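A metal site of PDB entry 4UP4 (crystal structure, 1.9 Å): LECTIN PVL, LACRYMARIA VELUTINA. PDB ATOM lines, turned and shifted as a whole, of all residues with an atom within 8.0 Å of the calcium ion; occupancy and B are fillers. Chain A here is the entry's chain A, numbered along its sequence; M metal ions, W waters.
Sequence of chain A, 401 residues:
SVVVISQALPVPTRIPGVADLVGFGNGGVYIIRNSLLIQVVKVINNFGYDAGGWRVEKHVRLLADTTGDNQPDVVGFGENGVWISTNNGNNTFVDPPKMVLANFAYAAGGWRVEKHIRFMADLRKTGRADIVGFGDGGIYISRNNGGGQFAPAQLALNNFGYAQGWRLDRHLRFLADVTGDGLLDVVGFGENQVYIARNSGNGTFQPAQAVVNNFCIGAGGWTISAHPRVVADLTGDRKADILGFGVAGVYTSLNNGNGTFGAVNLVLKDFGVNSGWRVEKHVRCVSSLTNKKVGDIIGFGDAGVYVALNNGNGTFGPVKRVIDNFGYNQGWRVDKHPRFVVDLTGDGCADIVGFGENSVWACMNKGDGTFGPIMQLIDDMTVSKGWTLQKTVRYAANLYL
The calcium ion is bound by OD1 of Asp 181 (2.4 Å), O of Leu 183 (2.4 Å), OD1 of Asp 177 (2.4 Å), OG1 of Thr 179 (2.6 Å), OD2 of Asp 185 (2.6 Å) and water W1 (2.6 Å). The calcium ion has six donor atoms within binding distance. Slightly farther from the calcium ion lies the side-chain carboxylate (OD1) of Asp 185 (3.1 Å).
Of the 18 residues printed, 5 come within 4 Å of the calcium ion. The nearest printed residue that does not touch the calcium ion is Val 178 (4.2 Å).
OD1 of Asp 185 is in hydrogen-bond range of N of Asn 199, 3.0 Å away. N of Gly 182 is in hydrogen-bond range of OD2 of Asp 177 (2.7 Å). O of Ala 176 sits at hydrogen-bond distance from N of Asp 185. The side-chain carboxylate of Asp 177 sits close to the backbone NH of Gly 180 (3.4 Å). The side-chain amino group (NZ) of Lys 125 sits at hydrogen-bond distance from the backbone carbonyl oxygen (O) of Asp 181. The side-chain carboxylate (OD2) of Asp 185 sits close to the backbone NH (N) of Val 178.
Water W1 bridges OD1 of Asp 185 and OD2 of Asp 181.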
ATOM      1  N   LYS A 125       2.949  -0.352  35.134  1.00  0.00           N
ATOM      2  CA  LYS A 125       1.725   0.433  35.184  1.00  0.00           C
ATOM      3  C   LYS A 125       0.915   0.138  36.416  1.00  0.00           C
ATOM      4  O   LYS A 125      -0.264  -0.204  36.315  1.00  0.00           O
ATOM      5  CB  LYS A 125       0.867   0.190  33.928  1.00  0.00           C
ATOM      6  CG  LYS A 125       1.453   0.557  32.605  1.00  0.00           C
ATOM      7  CD  LYS A 125       0.538   0.006  31.496  1.00  0.00           C
ATOM      8  CE  LYS A 125       0.702   0.721  30.187  1.00  0.00           C
ATOM      9  NZ  LYS A 125      -0.510   0.614  29.309  1.00  0.00           N
ATOM     10  N   ALA A 176      12.077   4.885  28.248  1.00  0.00           N
ATOM     11  CA  ALA A 176      11.127   5.547  27.321  1.00  0.00           C
ATOM     12  C   ALA A 176      10.280   4.519  26.595  1.00  0.00           C
ATOM     13  O   ALA A 176      10.774   3.460  26.213  1.00  0.00           O
ATOM     14  CB  ALA A 176      11.866   6.468  26.353  1.00  0.00           C
ATOM     15  N   ASP A 177       8.995   4.826  26.393  1.00  0.00           N
ATOM     16  CA  ASP A 177       8.133   3.959  25.639  1.00  0.00           C
ATOM     17  C   ASP A 177       8.456   4.152  24.143  1.00  0.00           C
ATOM     18  O   ASP A 177       8.112   5.209  23.608  1.00  0.00           O
ATOM     19  CB  ASP A 177       6.662   4.323  25.874  1.00  0.00           C
ATOM     20  CG  ASP A 177       5.677   3.394  25.116  1.00  0.00           C
ATOM     21  OD1 ASP A 177       6.113   2.396  24.482  1.00  0.00           O
ATOM     22  OD2 ASP A 177       4.478   3.645  25.189  1.00  0.00           O
ATOM     23  N   VAL A 178       9.114   3.126  23.532  1.00  0.00           N
ATOM     24  CA  VAL A 178       9.361   3.073  22.107  1.00  0.00           C
ATOM     25  C   VAL A 178       8.363   2.247  21.282  1.00  0.00           C
ATOM     26  O   VAL A 178       8.528   2.169  20.061  1.00  0.00           O
ATOM     27  CB  VAL A 178      10.819   2.608  21.771  1.00  0.00           C
ATOM     28  CG1 VAL A 178      11.826   3.555  22.397  1.00  0.00           C
ATOM     29  CG2 VAL A 178      11.091   1.174  22.169  1.00  0.00           C
ATOM     30  N   THR A 179       7.362   1.652  21.916  1.00  0.00           N
ATOM     31  CA  THR A 179       6.384   0.794  21.232  1.00  0.00           C
ATOM     32  C   THR A 179       4.949   1.335  21.190  1.00  0.00           C
ATOM     33  O   THR A 179       4.184   0.982  20.326  1.00  0.00           O
ATOM     34  CB  THR A 179       6.366  -0.653  21.810  1.00  0.00           C
ATOM     35  OG1 THR A 179       5.992  -0.617  23.154  1.00  0.00           O
ATOM     36  CG2 THR A 179       7.714  -1.284  21.778  1.00  0.00           C
ATOM     37  N   GLY A 180       4.584   2.234  22.106  1.00  0.00           N
ATOM     38  CA  GLY A 180       3.210   2.742  22.254  1.00  0.00           C
ATOM     39  C   GLY A 180       2.311   2.057  23.283  1.00  0.00           C
ATOM     40  O   GLY A 180       1.208   2.519  23.539  1.00  0.00           O
ATOM     41  N   ASP A 181       2.769   0.968  23.893  1.00  0.00           N
ATOM     42  CA  ASP A 181       1.956   0.229  24.843  1.00  0.00           C
ATOM     43  C   ASP A 181       1.934   0.897  26.217  1.00  0.00           C
ATOM     44  O   ASP A 181       1.269   0.431  27.160  1.00  0.00           O
ATOM     45  CB  ASP A 181       2.449  -1.222  24.936  1.00  0.00           C
ATOM     46  CG  ASP A 181       3.847  -1.344  25.535  1.00  0.00           C
ATOM     47  OD1 ASP A 181       4.469  -0.320  25.978  1.00  0.00           O
ATOM     48  OD2 ASP A 181       4.323  -2.489  25.572  1.00  0.00           O
ATOM     49  N   GLY A 182       2.666   2.004  26.333  1.00  0.00           N
ATOM     50  CA  GLY A 182       2.635   2.733  27.556  1.00  0.00           C
ATOM     51  C   GLY A 182       3.604   2.165  28.580  1.00  0.00           C
ATOM     52  O   GLY A 182       3.638   2.653  29.728  1.00  0.00           O
ATOM     53  N   LEU A 183       4.381   1.144  28.211  1.00  0.00           N
ATOM     54  CA  LEU A 183       5.402   0.631  29.145  1.00  0.00           C
ATOM     55  C   LEU A 183       6.774   1.230  28.768  1.00  0.00           C
ATOM     56  O   LEU A 183       7.117   1.325  27.578  1.00  0.00           O
ATOM     57  CB  LEU A 183       5.492  -0.869  29.142  1.00  0.00           C
ATOM     58  CG  LEU A 183       4.309  -1.646  29.756  1.00  0.00           C
ATOM     59  CD1 LEU A 183       4.306  -3.085  29.221  1.00  0.00           C
ATOM     60  CD2 LEU A 183       4.380  -1.633  31.269  1.00  0.00           C
ATOM     61  N   LEU A 184       7.517   1.688  29.773  1.00  0.00           N
ATOM     62  CA  LEU A 184       8.844   2.293  29.466  1.00  0.00           C
ATOM     63  C   LEU A 184       9.791   1.154  29.130  1.00  0.00           C
ATOM     64  O   LEU A 184       9.919   0.203  29.925  1.00  0.00           O
ATOM     65  CB  LEU A 184       9.358   3.119  30.638  1.00  0.00           C
ATOM     66  CG  LEU A 184       8.478   4.267  31.126  1.00  0.00           C
ATOM     67  CD1 LEU A 184       9.019   4.837  32.420  1.00  0.00           C
ATOM     68  CD2 LEU A 184       8.416   5.367  30.067  1.00  0.00           C
ATOM     69  N   ASP A 185      10.393   1.255  27.955  1.00  0.00           N
ATOM     70  CA  ASP A 185      11.408   0.350  27.469  1.00  0.00           C
ATOM     71  C   ASP A 185      12.798   0.951  27.724  1.00  0.00           C
ATOM     72  O   ASP A 185      12.910   2.162  28.064  1.00  0.00           O
ATOM     73  CB  ASP A 185      11.217   0.234  25.974  1.00  0.00           C
ATOM     74  CG  ASP A 185       9.829  -0.080  25.603  1.00  0.00           C
ATOM     75  OD1 ASP A 185       9.400  -1.172  26.042  1.00  0.00           O
ATOM     76  OD2 ASP A 185       9.183   0.703  24.872  1.00  0.00           O
ATOM     77  N   VAL A 186      13.837   0.120  27.636  1.00  0.00           N
ATOM     78  CA  VAL A 186      15.222   0.624  27.729  1.00  0.00           C
ATOM     79  C   VAL A 186      15.691   1.138  26.413  1.00  0.00           C
ATOM     80  O   VAL A 186      15.429   0.531  25.421  1.00  0.00           O
ATOM     81  CB  VAL A 186      16.219  -0.444  28.201  1.00  0.00           C
ATOM     82  CG1 VAL A 186      17.638   0.176  28.242  1.00  0.00           C
ATOM     83  CG2 VAL A 186      15.819  -1.006  29.563  1.00  0.00           C
ATOM     84  N   ALA A 197      15.399  -2.419  24.628  1.00  0.00           N
ATOM     85  CA  ALA A 197      14.982  -3.637  25.278  1.00  0.00           C
ATOM     86  C   ALA A 197      13.515  -3.424  25.709  1.00  0.00           C
ATOM     87  O   ALA A 197      13.210  -2.504  26.487  1.00  0.00           O
ATOM     88  CB  ALA A 197      15.883  -3.921  26.482  1.00  0.00           C
ATOM     89  N   ARG A 198      12.635  -4.295  25.225  1.00  0.00           N
ATOM     90  CA  ARG A 198      11.236  -4.142  25.413  1.00  0.00           C
ATOM     91  C   ARG A 198      10.785  -4.599  26.794  1.00  0.00           C
ATOM     92  O   ARG A 198      11.076  -5.683  27.176  1.00  0.00           O
ATOM     93  CB  ARG A 198      10.488  -4.899  24.338  1.00  0.00           C
ATOM     94  CG  ARG A 198      10.714  -4.301  22.955  1.00  0.00           C
ATOM     95  CD  ARG A 198      10.280  -5.256  21.858  1.00  0.00           C
ATOM     96  NE  ARG A 198      10.722  -4.808  20.524  1.00  0.00           N
ATOM     97  CZ  ARG A 198       9.971  -4.160  19.635  1.00  0.00           C
ATOM     98  NH1 ARG A 198       8.705  -3.924  19.896  1.00  0.00           N
ATOM     99  NH2 ARG A 198      10.489  -3.756  18.459  1.00  0.00           N
ATOM    100  N   ASN A 199      10.053  -3.731  27.476  1.00  0.00           N
ATOM    101  CA  ASN A 199       9.447  -3.988  28.736  1.00  0.00           C
ATOM    102  C   ASN A 199       8.337  -4.965  28.562  1.00  0.00           C
ATOM    103  O   ASN A 199       7.430  -4.738  27.768  1.00  0.00           O
ATOM    104  CB  ASN A 199       8.895  -2.654  29.302  1.00  0.00           C
ATOM    105  CG  ASN A 199       8.409  -2.769  30.749  1.00  0.00           C
ATOM    106  OD1 ASN A 199       7.967  -3.849  31.175  1.00  0.00           O
ATOM    107  ND2 ASN A 199       8.456  -1.634  31.522  1.00  0.00           N
ATOM    108  N   SER A 200       8.413  -6.065  29.261  1.00  0.00           N
ATOM    109  CA  SER A 200       7.359  -7.071  29.155  1.00  0.00           C
ATOM    110  C   SER A 200       6.261  -6.869  30.149  1.00  0.00           C
ATOM    111  O   SER A 200       5.272  -7.607  30.143  1.00  0.00           O
ATOM    112  CB  SER A 200       7.937  -8.482  29.309  1.00  0.00           C
ATOM    113  OG  SER A 200       8.824  -8.779  28.276  1.00  0.00           O
ATOM    114  N   ARG A 238       3.225   9.771  20.734  1.00  0.00           N
ATOM    115  CA  ARG A 238       3.613   9.225  22.066  1.00  0.00           C
ATOM    116  C   ARG A 238       4.639   8.091  22.037  1.00  0.00           C
ATOM    117  O   ARG A 238       4.906   7.458  23.093  1.00  0.00           O
ATOM    118  CB  ARG A 238       2.373   8.796  22.861  1.00  0.00           C
ATOM    119  CG  ARG A 238       1.267   9.827  22.911  1.00  0.00           C
ATOM    120  CD  ARG A 238       0.081   9.404  23.785  1.00  0.00           C
ATOM    121  NE  ARG A 238       0.203  10.090  25.083  1.00  0.00           N
ATOM    122  CZ  ARG A 238      -0.004  11.407  25.228  1.00  0.00           C
ATOM    123  NH1 ARG A 238      -0.364  12.160  24.181  1.00  0.00           N
ATOM    124  NH2 ARG A 238       0.147  11.989  26.415  1.00  0.00           N
ATOM    125  N   LYS A 239       5.236   7.854  20.873  1.00  0.00           N
ATOM    126  CA  LYS A 239       6.341   6.903  20.720  1.00  0.00           C
ATOM    127  C   LYS A 239       7.656   7.692  20.617  1.00  0.00           C
ATOM    128  O   LYS A 239       7.762   8.643  19.882  1.00  0.00           O
ATOM    129  CB  LYS A 239       6.117   6.033  19.500  1.00  0.00           C
ATOM    130  CG  LYS A 239       4.892   5.137  19.632  1.00  0.00           C
ATOM    131  CD  LYS A 239       4.482   4.468  18.340  1.00  0.00           C
ATOM    132  CE  LYS A 239       3.092   3.865  18.438  1.00  0.00           C
ATOM    133  NZ  LYS A 239       2.784   3.106  17.232  1.00  0.00           N
HETATM  134 CA    CA M   1       6.695   0.241  25.468  1.00  0.00          CA
HETATM  135  O   HOH W   1       7.155  -2.284  25.038  1.00  0.00           O
